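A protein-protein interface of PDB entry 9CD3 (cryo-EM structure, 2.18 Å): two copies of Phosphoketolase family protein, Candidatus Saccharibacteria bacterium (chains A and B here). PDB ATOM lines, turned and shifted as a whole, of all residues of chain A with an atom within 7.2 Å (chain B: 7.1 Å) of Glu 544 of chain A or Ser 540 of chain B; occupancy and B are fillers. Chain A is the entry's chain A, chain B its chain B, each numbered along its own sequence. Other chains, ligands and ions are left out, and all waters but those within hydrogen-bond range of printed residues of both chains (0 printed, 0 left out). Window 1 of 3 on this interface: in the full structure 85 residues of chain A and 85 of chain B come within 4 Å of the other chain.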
ATOM      1  N   PRO A 490       3.328  22.605  -7.380  1.00  0.00           N
ATOM      2  CA  PRO A 490       3.260  21.242  -6.821  1.00  0.00           C
ATOM      3  C   PRO A 490       1.950  20.878  -6.130  1.00  0.00           C
ATOM      4  O   PRO A 490       1.825  19.771  -5.600  1.00  0.00           O
ATOM      5  CB  PRO A 490       4.422  21.222  -5.818  1.00  0.00           C
ATOM      6  CG  PRO A 490       5.362  22.237  -6.312  1.00  0.00           C
ATOM      7  CD  PRO A 490       4.507  23.327  -6.868  1.00  0.00           C
ATOM      8  N   ILE A 492      -0.799  20.277  -7.630  1.00  0.00           N
ATOM      9  CA  ILE A 492      -1.484  19.311  -8.482  1.00  0.00           C
ATOM     10  C   ILE A 492      -0.509  18.230  -8.926  1.00  0.00           C
ATOM     11  O   ILE A 492      -0.645  17.667 -10.016  1.00  0.00           O
ATOM     12  CB  ILE A 492      -2.123  20.005  -9.696  1.00  0.00           C
ATOM     13  CG1 ILE A 492      -1.075  20.843 -10.431  1.00  0.00           C
ATOM     14  CG2 ILE A 492      -3.290  20.872  -9.260  1.00  0.00           C
ATOM     15  CD1 ILE A 492      -1.398  21.104 -11.877  1.00  0.00           C
ATOM     16  N   SER A 493       0.480  17.935  -8.081  1.00  0.00           N
ATOM     17  CA  SER A 493       1.501  16.957  -8.440  1.00  0.00           C
ATOM     18  C   SER A 493       0.907  15.566  -8.640  1.00  0.00           C
ATOM     19  O   SER A 493       1.308  14.838  -9.555  1.00  0.00           O
ATOM     20  CB  SER A 493       2.591  16.931  -7.371  1.00  0.00           C
ATOM     21  OG  SER A 493       3.302  15.708  -7.402  1.00  0.00           O
ATOM     22  N   SER A 494      -0.047  15.175  -7.792  1.00  0.00           N
ATOM     23  CA  SER A 494      -0.594  13.822  -7.870  1.00  0.00           C
ATOM     24  C   SER A 494      -1.464  13.636  -9.109  1.00  0.00           C
ATOM     25  O   SER A 494      -1.455  12.562  -9.720  1.00  0.00           O
ATOM     26  CB  SER A 494      -1.386  13.502  -6.605  1.00  0.00           C
ATOM     27  OG  SER A 494      -2.320  14.526  -6.315  1.00  0.00           O
ATOM     28  N   MET A 496      -1.154  15.081 -12.058  1.00  0.00           N
ATOM     29  CA  MET A 496      -0.290  14.896 -13.218  1.00  0.00           C
ATOM     30  C   MET A 496       0.229  13.465 -13.289  1.00  0.00           C
ATOM     31  O   MET A 496       0.422  12.920 -14.382  1.00  0.00           O
ATOM     32  CB  MET A 496       0.870  15.891 -13.170  1.00  0.00           C
ATOM     33  CG  MET A 496       1.851  15.769 -14.320  1.00  0.00           C
ATOM     34  SD  MET A 496       3.421  15.042 -13.817  1.00  0.00           S
ATOM     35  CE  MET A 496       3.728  15.920 -12.287  1.00  0.00           C
ATOM     36  N   ASP A 497       0.461  12.840 -12.132  1.00  0.00           N
ATOM     37  CA  ASP A 497       0.939  11.461 -12.119  1.00  0.00           C
ATOM     38  C   ASP A 497      -0.127  10.496 -12.627  1.00  0.00           C
ATOM     39  O   ASP A 497       0.187   9.527 -13.327  1.00  0.00           O
ATOM     40  CB  ASP A 497       1.384  11.073 -10.710  1.00  0.00           C
ATOM     41  CG  ASP A 497       2.722  11.670 -10.344  1.00  0.00           C
ATOM     42  OD1 ASP A 497       3.501  11.977 -11.267  1.00  0.00           O
ATOM     43  OD2 ASP A 497       2.999  11.828  -9.139  1.00  0.00           O
ATOM     44  N   PRO A 539      10.897  25.038  -6.195  1.00  0.00           N
ATOM     45  CA  PRO A 539      11.078  24.465  -7.534  1.00  0.00           C
ATOM     46  C   PRO A 539      11.077  22.936  -7.557  1.00  0.00           C
ATOM     47  O   PRO A 539      12.013  22.299  -8.052  1.00  0.00           O
ATOM     48  CB  PRO A 539      12.437  25.031  -7.956  1.00  0.00           C
ATOM     49  CG  PRO A 539      13.196  25.128  -6.667  1.00  0.00           C
ATOM     50  CD  PRO A 539      12.188  25.335  -5.552  1.00  0.00           C
ATOM     51  N   SER A 540      10.013  22.330  -7.030  1.00  0.00           N
ATOM     52  CA  SER A 540       9.939  20.877  -6.932  1.00  0.00           C
ATOM     53  C   SER A 540       9.075  20.230  -8.007  1.00  0.00           C
ATOM     54  O   SER A 540       9.186  19.018  -8.216  1.00  0.00           O
ATOM     55  CB  SER A 540       9.406  20.464  -5.554  1.00  0.00           C
ATOM     56  OG  SER A 540       8.299  21.259  -5.172  1.00  0.00           O
ATOM     57  N   PHE A 541       8.226  21.001  -8.692  1.00  0.00           N
ATOM     58  CA  PHE A 541       7.310  20.414  -9.666  1.00  0.00           C
ATOM     59  C   PHE A 541       8.054  19.807 -10.849  1.00  0.00           C
ATOM     60  O   PHE A 541       7.669  18.745 -11.351  1.00  0.00           O
ATOM     61  CB  PHE A 541       6.309  21.463 -10.144  1.00  0.00           C
ATOM     62  CG  PHE A 541       5.334  20.949 -11.160  1.00  0.00           C
ATOM     63  CD1 PHE A 541       4.202  20.257 -10.766  1.00  0.00           C
ATOM     64  CD2 PHE A 541       5.544  21.159 -12.512  1.00  0.00           C
ATOM     65  CE1 PHE A 541       3.303  19.782 -11.700  1.00  0.00           C
ATOM     66  CE2 PHE A 541       4.648  20.688 -13.451  1.00  0.00           C
ATOM     67  CZ  PHE A 541       3.527  19.999 -13.045  1.00  0.00           C
ATOM     68  N   ILE A 542       9.113  20.469 -11.319  1.00  0.00           N
ATOM     69  CA  ILE A 542       9.845  19.962 -12.479  1.00  0.00           C
ATOM     70  C   ILE A 542      10.528  18.640 -12.147  1.00  0.00           C
ATOM     71  O   ILE A 542      10.645  17.752 -13.004  1.00  0.00           O
ATOM     72  CB  ILE A 542      10.845  21.016 -12.992  1.00  0.00           C
ATOM     73  CG1 ILE A 542      11.890  21.354 -11.928  1.00  0.00           C
ATOM     74  CG2 ILE A 542      10.112  22.271 -13.427  1.00  0.00           C
ATOM     75  CD1 ILE A 542      13.158  21.955 -12.492  1.00  0.00           C
ATOM     76  N   ASP A 543      10.990  18.485 -10.904  1.00  0.00           N
ATOM     77  CA  ASP A 543      11.575  17.216 -10.482  1.00  0.00           C
ATOM     78  C   ASP A 543      10.540  16.100 -10.536  1.00  0.00           C
ATOM     79  O   ASP A 543      10.844  14.970 -10.937  1.00  0.00           O
ATOM     80  CB  ASP A 543      12.157  17.352  -9.073  1.00  0.00           C
ATOM     81  CG  ASP A 543      13.154  16.256  -8.738  1.00  0.00           C
ATOM     82  OD1 ASP A 543      13.208  15.243  -9.465  1.00  0.00           O
ATOM     83  OD2 ASP A 543      13.889  16.407  -7.741  1.00  0.00           O
ATOM     84  N   GLU A 544       9.303  16.400 -10.135  1.00  0.00           N
ATOM     85  CA  GLU A 544       8.241  15.402 -10.201  1.00  0.00           C
ATOM     86  C   GLU A 544       7.929  15.022 -11.644  1.00  0.00           C
ATOM     87  O   GLU A 544       7.655  13.853 -11.939  1.00  0.00           O
ATOM     88  CB  GLU A 544       6.990  15.924  -9.496  1.00  0.00           C
ATOM     89  CG  GLU A 544       5.849  14.924  -9.427  1.00  0.00           C
ATOM     90  CD  GLU A 544       5.873  14.092  -8.159  1.00  0.00           C
ATOM     91  OE1 GLU A 544       6.948  13.993  -7.531  1.00  0.00           O
ATOM     92  OE2 GLU A 544       4.817  13.540  -7.787  1.00  0.00           O
ATOM     93  N   VAL A 545       7.959  15.997 -12.556  1.00  0.00           N
ATOM     94  CA  VAL A 545       7.690  15.712 -13.963  1.00  0.00           C
ATOM     95  C   VAL A 545       8.805  14.872 -14.568  1.00  0.00           C
ATOM     96  O   VAL A 545       8.542  13.948 -15.348  1.00  0.00           O
ATOM     97  CB  VAL A 545       7.481  17.026 -14.740  1.00  0.00           C
ATOM     98  CG1 VAL A 545       7.586  16.792 -16.239  1.00  0.00           C
ATOM     99  CG2 VAL A 545       6.135  17.631 -14.397  1.00  0.00           C
ATOM    100  N   LEU A 546      10.057  15.151 -14.213  1.00  0.00           N
ATOM    101  CA  LEU A 546      11.190  14.403 -14.744  1.00  0.00           C
ATOM    102  C   LEU A 546      11.265  12.970 -14.230  1.00  0.00           C
ATOM    103  O   LEU A 546      12.236  12.273 -14.538  1.00  0.00           O
ATOM    104  CB  LEU A 546      12.497  15.127 -14.413  1.00  0.00           C
ATOM    105  CG  LEU A 546      12.926  16.267 -15.337  1.00  0.00           C
ATOM    106  CD1 LEU A 546      13.791  17.259 -14.584  1.00  0.00           C
ATOM    107  CD2 LEU A 546      13.667  15.719 -16.543  1.00  0.00           C
ATOM    108  N   ARG A 547      10.273  12.510 -13.469  1.00  0.00           N
ATOM    109  CA  ARG A 547      10.366  11.231 -12.780  1.00  0.00           C
ATOM    110  C   ARG A 547       9.646  10.096 -13.499  1.00  0.00           C
ATOM    111  O   ARG A 547       9.912   8.928 -13.199  1.00  0.00           O
ATOM    112  CB  ARG A 547       9.808  11.373 -11.363  1.00  0.00           C
ATOM    113  CG  ARG A 547      10.401  10.423 -10.344  1.00  0.00           C
ATOM    114  CD  ARG A 547      11.509  11.103  -9.547  1.00  0.00           C
ATOM    115  NE  ARG A 547      11.053  12.231  -8.737  1.00  0.00           N
ATOM    116  CZ  ARG A 547      10.042  12.213  -7.874  1.00  0.00           C
ATOM    117  NH1 ARG A 547       9.375  11.105  -7.603  1.00  0.00           N
ATOM    118  NH2 ARG A 547       9.706  13.338  -7.251  1.00  0.00           N
ATOM    119  N   ARG A 548       8.742  10.405 -14.427  1.00  0.00           N
ATOM    120  CA  ARG A 548       8.087   9.366 -15.211  1.00  0.00           C
ATOM    121  C   ARG A 548       9.092   8.704 -16.148  1.00  0.00           C
ATOM    122  O   ARG A 548       9.956   9.369 -16.727  1.00  0.00           O
ATOM    123  CB  ARG A 548       6.925   9.955 -16.008  1.00  0.00           C
ATOM    124  CG  ARG A 548       6.257  11.151 -15.350  1.00  0.00           C
ATOM    125  CD  ARG A 548       5.511  10.740 -14.096  1.00  0.00           C
ATOM    126  NE  ARG A 548       6.283  10.986 -12.884  1.00  0.00           N
ATOM    127  CZ  ARG A 548       5.990  10.476 -11.696  1.00  0.00           C
ATOM    128  NH1 ARG A 548       4.962   9.661 -11.528  1.00  0.00           N
ATOM    129  NH2 ARG A 548       6.742  10.796 -10.648  1.00  0.00           N
ATOM    130  N   THR A 705      18.080  17.366  -8.037  1.00  0.00           N
ATOM    131  CA  THR A 705      17.367  17.085  -9.279  1.00  0.00           C
ATOM    132  C   THR A 705      18.338  16.879 -10.434  1.00  0.00           C
ATOM    133  O   THR A 705      18.151  15.979 -11.260  1.00  0.00           O
ATOM    134  CB  THR A 705      16.391  18.218  -9.595  1.00  0.00           C
ATOM    135  OG1 THR A 705      15.486  18.387  -8.499  1.00  0.00           O
ATOM    136  CG2 THR A 705      15.600  17.908 -10.850  1.00  0.00           C
ATOM    137  N   GLU B 486       0.422   4.457   0.599  1.00  0.00           N
ATOM    138  CA  GLU B 486       1.639   5.117   0.140  1.00  0.00           C
ATOM    139  C   GLU B 486       1.427   5.853  -1.177  1.00  0.00           C
ATOM    140  O   GLU B 486       1.936   6.967  -1.349  1.00  0.00           O
ATOM    141  CB  GLU B 486       2.773   4.103   0.001  1.00  0.00           C
ATOM    142  CG  GLU B 486       3.796   4.472  -1.051  1.00  0.00           C
ATOM    143  CD  GLU B 486       5.172   3.921  -0.750  1.00  0.00           C
ATOM    144  OE1 GLU B 486       5.326   2.683  -0.726  1.00  0.00           O
ATOM    145  OE2 GLU B 486       6.101   4.728  -0.540  1.00  0.00           O
ATOM    146  N   ALA B 487       0.674   5.261  -2.106  1.00  0.00           N
ATOM    147  CA  ALA B 487       0.528   5.851  -3.432  1.00  0.00           C
ATOM    148  C   ALA B 487      -0.229   7.173  -3.398  1.00  0.00           C
ATOM    149  O   ALA B 487      -0.037   8.015  -4.280  1.00  0.00           O
ATOM    150  CB  ALA B 487      -0.170   4.867  -4.369  1.00  0.00           C
ATOM    151  N   ALA B 489      -0.164   9.352  -0.779  1.00  0.00           N
ATOM    152  CA  ALA B 489       0.512  10.369   0.022  1.00  0.00           C
ATOM    153  C   ALA B 489       0.848  11.645  -0.746  1.00  0.00           C
ATOM    154  O   ALA B 489       0.680  12.734  -0.168  1.00  0.00           O
ATOM    155  CB  ALA B 489       1.775   9.770   0.653  1.00  0.00           C
ATOM    156  N   PRO B 490       1.326  11.609  -2.000  1.00  0.00           N
ATOM    157  CA  PRO B 490       1.726  12.862  -2.670  1.00  0.00           C
ATOM    158  C   PRO B 490       0.617  13.899  -2.822  1.00  0.00           C
ATOM    159  O   PRO B 490       0.890  14.983  -3.351  1.00  0.00           O
ATOM    160  CB  PRO B 490       2.219  12.384  -4.041  1.00  0.00           C
ATOM    161  CG  PRO B 490       2.651  10.998  -3.816  1.00  0.00           C
ATOM    162  CD  PRO B 490       1.697  10.436  -2.813  1.00  0.00           C
ATOM    163  N   SER B 493       1.785  16.981  -0.724  1.00  0.00           N
ATOM    164  CA  SER B 493       3.202  17.322  -0.816  1.00  0.00           C
ATOM    165  C   SER B 493       3.443  18.800  -0.536  1.00  0.00           C
ATOM    166  O   SER B 493       4.408  19.159   0.148  1.00  0.00           O
ATOM    167  CB  SER B 493       3.746  16.949  -2.194  1.00  0.00           C
ATOM    168  OG  SER B 493       3.193  15.730  -2.646  1.00  0.00           O
ATOM    169  N   GLN B 537       0.255   2.518  -7.365  1.00  0.00           N
ATOM    170  CA  GLN B 537       1.698   2.281  -7.268  1.00  0.00           C
ATOM    171  C   GLN B 537       2.420   3.582  -7.609  1.00  0.00           C
ATOM    172  O   GLN B 537       2.631   3.888  -8.787  1.00  0.00           O
ATOM    173  CB  GLN B 537       2.134   1.146  -8.189  1.00  0.00           C
ATOM    174  CG  GLN B 537       1.250  -0.093  -8.139  1.00  0.00           C
ATOM    175  CD  GLN B 537       1.447  -1.009  -9.329  1.00  0.00           C
ATOM    176  OE1 GLN B 537       2.317  -0.781 -10.167  1.00  0.00           O
ATOM    177  NE2 GLN B 537       0.635  -2.056  -9.408  1.00  0.00           N
ATOM    178  N   ASN B 538       2.814   4.338  -6.579  1.00  0.00           N
ATOM    179  CA  ASN B 538       3.442   5.639  -6.773  1.00  0.00           C
ATOM    180  C   ASN B 538       4.283   6.025  -5.561  1.00  0.00           C
ATOM    181  O   ASN B 538       3.792   6.715  -4.660  1.00  0.00           O
ATOM    182  CB  ASN B 538       2.377   6.703  -7.042  1.00  0.00           C
ATOM    183  CG  ASN B 538       2.970   8.031  -7.472  1.00  0.00           C
ATOM    184  OD1 ASN B 538       4.085   8.088  -7.986  1.00  0.00           O
ATOM    185  ND2 ASN B 538       2.220   9.105  -7.265  1.00  0.00           N
ATOM    186  N   PRO B 539       5.554   5.603  -5.498  1.00  0.00           N
ATOM    187  CA  PRO B 539       6.414   5.902  -4.346  1.00  0.00           C
ATOM    188  C   PRO B 539       7.197   7.207  -4.483  1.00  0.00           C
ATOM    189  O   PRO B 539       8.430   7.228  -4.402  1.00  0.00           O
ATOM    190  CB  PRO B 539       7.348   4.689  -4.307  1.00  0.00           C
ATOM    191  CG  PRO B 539       7.507   4.323  -5.752  1.00  0.00           C
ATOM    192  CD  PRO B 539       6.239   4.744  -6.477  1.00  0.00           C
ATOM    193  N   SER B 540       6.484   8.316  -4.678  1.00  0.00           N
ATOM    194  CA  SER B 540       7.134   9.601  -4.902  1.00  0.00           C
ATOM    195  C   SER B 540       7.153  10.504  -3.675  1.00  0.00           C
ATOM    196  O   SER B 540       7.925  11.468  -3.652  1.00  0.00           O
ATOM    197  CB  SER B 540       6.456  10.342  -6.062  1.00  0.00           C
ATOM    198  OG  SER B 540       5.270  10.990  -5.642  1.00  0.00           O
ATOM    199  N   PHE B 541       6.332  10.219  -2.661  1.00  0.00           N
ATOM    200  CA  PHE B 541       6.269  11.089  -1.489  1.00  0.00           C
ATOM    201  C   PHE B 541       7.581  11.092  -0.715  1.00  0.00           C
ATOM    202  O   PHE B 541       8.020  12.142  -0.234  1.00  0.00           O
ATOM    203  CB  PHE B 541       5.116  10.668  -0.579  1.00  0.00           C
ATOM    204  CG  PHE B 541       4.992  11.499   0.664  1.00  0.00           C
ATOM    205  CD1 PHE B 541       4.332  12.715   0.637  1.00  0.00           C
ATOM    206  CD2 PHE B 541       5.534  11.064   1.862  1.00  0.00           C
ATOM    207  CE1 PHE B 541       4.217  13.482   1.780  1.00  0.00           C
ATOM    208  CE2 PHE B 541       5.421  11.827   3.008  1.00  0.00           C
ATOM    209  CZ  PHE B 541       4.762  13.036   2.967  1.00  0.00           C
ATOM    210  N   ILE B 542       8.218   9.927  -0.569  1.00  0.00           N
ATOM    211  CA  ILE B 542       9.457   9.858   0.201  1.00  0.00           C
ATOM    212  C   ILE B 542      10.573  10.629  -0.491  1.00  0.00           C
ATOM    213  O   ILE B 542      11.513  11.095   0.164  1.00  0.00           O
ATOM    214  CB  ILE B 542       9.857   8.392   0.462  1.00  0.00           C
ATOM    215  CG1 ILE B 542      10.313   7.708  -0.828  1.00  0.00           C
ATOM    216  CG2 ILE B 542       8.704   7.634   1.095  1.00  0.00           C
ATOM    217  CD1 ILE B 542      11.031   6.399  -0.602  1.00  0.00           C
ATOM    218  N   ASP B 543      10.502  10.771  -1.816  1.00  0.00           N
ATOM    219  CA  ASP B 543      11.479  11.596  -2.520  1.00  0.00           C
ATOM    220  C   ASP B 543      11.289  13.071  -2.184  1.00  0.00           C
ATOM    221  O   ASP B 543      12.268  13.815  -2.046  1.00  0.00           O
ATOM    222  CB  ASP B 543      11.373  11.366  -4.028  1.00  0.00           C
ATOM    223  CG  ASP B 543      12.620  11.804  -4.778  1.00  0.00           C
ATOM    224  OD1 ASP B 543      13.496  12.448  -4.166  1.00  0.00           O
ATOM    225  OD2 ASP B 543      12.724  11.502  -5.984  1.00  0.00           O
ATOM    226  N   GLU B 544      10.037  13.511  -2.050  1.00  0.00           N
ATOM    227  CA  GLU B 544       9.772  14.908  -1.724  1.00  0.00           C
ATOM    228  C   GLU B 544      10.278  15.262  -0.331  1.00  0.00           C
ATOM    229  O   GLU B 544      10.784  16.368  -0.110  1.00  0.00           O
ATOM    230  CB  GLU B 544       8.276  15.197  -1.845  1.00  0.00           C
ATOM    231  CG  GLU B 544       7.903  16.651  -1.613  1.00  0.00           C
ATOM    232  CD  GLU B 544       7.715  17.420  -2.906  1.00  0.00           C
ATOM    233  OE1 GLU B 544       8.184  16.938  -3.958  1.00  0.00           O
ATOM    234  OE2 GLU B 544       7.099  18.505  -2.874  1.00  0.00           O
ATOM    235  N   VAL B 545      10.145  14.337   0.624  1.00  0.00           N
ATOM    236  CA  VAL B 545      10.580  14.604   1.991  1.00  0.00           C
ATOM    237  C   VAL B 545      12.097  14.736   2.064  1.00  0.00           C
ATOM    238  O   VAL B 545      12.620  15.567   2.817  1.00  0.00           O
ATOM    239  CB  VAL B 545      10.054  13.503   2.932  1.00  0.00           C
ATOM    240  CG1 VAL B 545      10.763  13.547   4.277  1.00  0.00           C
ATOM    241  CG2 VAL B 545       8.554  13.645   3.121  1.00  0.00           C
ATOM    242  N   ARG B 547      14.131  16.060   0.075  1.00  0.00           N
ATOM    243  CA  ARG B 547      14.684  17.203  -0.642  1.00  0.00           C
ATOM    244  C   ARG B 547      14.831  18.452   0.217  1.00  0.00           C
ATOM    245  O   ARG B 547      15.410  19.438  -0.251  1.00  0.00           O
ATOM    246  CB  ARG B 547      13.822  17.521  -1.867  1.00  0.00           C
ATOM    247  CG  ARG B 547      14.111  16.626  -3.060  1.00  0.00           C
ATOM    248  CD  ARG B 547      13.821  17.338  -4.364  1.00  0.00           C
ATOM    249  NE  ARG B 547      12.393  17.564  -4.540  1.00  0.00           N
ATOM    250  CZ  ARG B 547      11.529  16.633  -4.914  1.00  0.00           C
ATOM    251  NH1 ARG B 547      11.917  15.396  -5.176  1.00  0.00           N
ATOM    252  NH2 ARG B 547      10.242  16.948  -5.026  1.00  0.00           N
ATOM    253  N   GLY B 701      11.715   2.237  -3.986  1.00  0.00           N
ATOM    254  CA  GLY B 701      11.113   3.304  -4.763  1.00  0.00           C
ATOM    255  C   GLY B 701      11.799   3.570  -6.088  1.00  0.00           C
ATOM    256  O   GLY B 701      12.414   2.672  -6.671  1.00  0.00           O
ATOM    257  N   TYR B 702      11.696   4.806  -6.571  1.00  0.00           N
ATOM    258  CA  TYR B 702      12.282   5.168  -7.854  1.00  0.00           C
ATOM    259  C   TYR B 702      13.800   5.071  -7.802  1.00  0.00           C
ATOM    260  O   TYR B 702      14.424   5.360  -6.778  1.00  0.00           O
ATOM    261  CB  TYR B 702      11.861   6.583  -8.246  1.00  0.00           C
ATOM    262  CG  TYR B 702      10.400   6.720  -8.602  1.00  0.00           C
ATOM    263  CD1 TYR B 702       9.869   6.059  -9.699  1.00  0.00           C
ATOM    264  CD2 TYR B 702       9.554   7.516  -7.847  1.00  0.00           C
ATOM    265  CE1 TYR B 702       8.538   6.184 -10.030  1.00  0.00           C
ATOM    266  CE2 TYR B 702       8.222   7.647  -8.170  1.00  0.00           C
ATOM    267  CZ  TYR B 702       7.718   6.978  -9.263  1.00  0.00           C
ATOM    268  OH  TYR B 702       6.389   7.103  -9.589  1.00  0.00           O
ATOM    269  N   LYS B 704      15.917   6.961  -9.340  1.00  0.00           N
ATOM    270  CA  LYS B 704      16.575   8.264  -9.326  1.00  0.00           C
ATOM    271  C   LYS B 704      16.638   8.854  -7.924  1.00  0.00           C
ATOM    272  O   LYS B 704      17.509   9.684  -7.644  1.00  0.00           O
ATOM    273  CB  LYS B 704      15.860   9.220 -10.280  1.00  0.00           C
ATOM    274  CG  LYS B 704      16.086   8.894 -11.747  1.00  0.00           C
ATOM    275  CD  LYS B 704      15.890  10.111 -12.633  1.00  0.00           C
ATOM    276  CE  LYS B 704      14.450  10.233 -13.097  1.00  0.00           C
ATOM    277  NZ  LYS B 704      13.599  10.916 -12.088  1.00  0.00           N
ATOM    278  N   THR B 705      15.728   8.446  -7.036  1.00  0.00           N
ATOM    279  CA  THR B 705      15.772   8.924  -5.657  1.00  0.00           C
ATOM    280  C   THR B 705      17.055   8.484  -4.963  1.00  0.00           C
ATOM    281  O   THR B 705      17.677   9.267  -4.236  1.00  0.00           O
ATOM    282  CB  THR B 705      14.551   8.423  -4.888  1.00  0.00           C
ATOM    283  OG1 THR B 705      13.359   8.831  -5.569  1.00  0.00           O
ATOM    284  CG2 THR B 705      14.538   8.987  -3.482  1.00  0.00           C
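Printed residues of chain B that touch a printed residue of chain A: Asn 538, Ser 540, Asp 543, Glu 544, Arg 547, Tyr 702 and Lys 704. Hydrophobic or aromatic side chains of chain B that line the printed part of chain A: Tyr 702. Among the printed residues, 13 pairs touch across the chains. Among the printed residues, Asp or Glu carboxylates within 4 Å of a Lys or Arg side-chain nitrogen of the other chain: Asp 543 of chain A with Arg 547 of chain B (3.4 Å) and Arg 547 of chain A with Asp 543 of chain B (3.3 Å).
Ser 540 of chain A touches Glu 544 of chain B. Ser 540 of chain A touches Arg 547 of chain B. NH1 of Arg 547 of chain A touches CB of Ser 540 of chain B, 3.4 Å away. NH1 of Arg 547 of chain B touches NH2 of Arg 547 of chain A (3.7 Å). Tyr 702 of chain B touches Arg 547 of chain A (CD2 to NH1, 3.6 Å). Arg 547 of chain A touches Lys 704 of chain B (CD to NZ, 3.3 Å). Arg 548 of chain A touches Asn 538 of chain B (NH1 to OD1, 3.97 Å). NH1 of Arg 548 of chain A touches OH of Tyr 702 of chain B, at 3.5 Å.
The side-chain amino group (NZ) of Lys 704 of chain B sits at hydrogen-bond distance from the backbone carbonyl oxygen (O) of Leu 546 of chain A (3.1 Å). The side-chain carboxylate (OE2) of Glu 544 of chain A lies within hydrogen-bond range of the side-chain hydroxyl (OG) of Ser 540 of chain B. NH1 of Arg 547 of chain B lies within salt-bridge range of OD2 of Asp 543 of chain A. The guanidinium group (NE) of Arg 547 of chain A is in salt-bridge range of the side-chain carboxylate (OD2) of Asp 543 of chain B (3.3 Å). The side-chain carboxylate (OD2) of Asp 497 of chain A sits at hydrogen-bond distance from the side-chain amide nitrogen (ND2) of Asn 538 of chain B.
The guanidinium group (NH1) of Arg 547 of chain B is in salt-bridge range of the side-chain carboxylate (OD1) of Asp 543 of chain B (3.5 Å). The side-chain carboxylate of Glu 544 of chain A is in salt-bridge range of the guanidinium group of Arg 547 of chain A (2.8 Å). O of Glu 544 of chain A lies within hydrogen-bond range of NE of Arg 548 of chain A, 3.3 Å away. The side-chain carboxylate of Asp 543 of chain A lies within hydrogen-bond range of the side-chain hydroxyl of Thr 705 of chain A, 2.7 Å away. The side-chain hydroxyl (OG1) of Thr 705 of chain B is in hydrogen-bond range of the side-chain carboxylate (OD2) of Asp 543 of chain B, at 2.8 Å. The side-chain carboxylate (OD1) of Asp 497 of chain A is in salt-bridge range of the guanidinium group (NH1) of Arg 548 of chain A, 2.8 Å away.
Glu 544 of chain A touches just one residue of chain B: Ser 540 (3.4 Å). Val 545 of chain A touches none of the printed residues of chain B. Printed residues of chain B within 4 Å of Arg 547 of chain A: Ser 540, Asp 543, Arg 547, Tyr 702 and Lys 704. Printed residues of chain A within 4 Å of Asn 538 of chain B: Asp 497 and Arg 548. Of the printed residues of chain A, Ser 540 of chain B touches Glu 544 and Arg 547. Of the printed residues of chain A, Tyr 702 of chain B touches Arg 547 and Arg 548. The nearest residue of chain B that does not touch Glu 544 of chain A is Pro 490 of chain B (4.7 Å).
Ser 540 of chain A touches Glu 544 of chain B, and with the chains exchanged Glu 544 of chain A touches Ser 540 of chain B. Ser 540 of chain A touches Arg 547 of chain B, and with the chains exchanged Arg 547 of chain A touches Ser 540 of chain B. Asp 543 of chain A touches Arg 547 of chain B, and with the chains exchanged Arg 547 of chain A touches Asp 543 of chain B. Arg 547 of chain A touches its own counterpart, Arg 547 of chain B. Positions printed for both chains: 490, 493, 539, 540, 541, 542, 543, 544, 545, 547 and 705. Of the 13 pairs that touch across the chains among the printed residues, 7 have their exchanged pair printed and touching as well.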
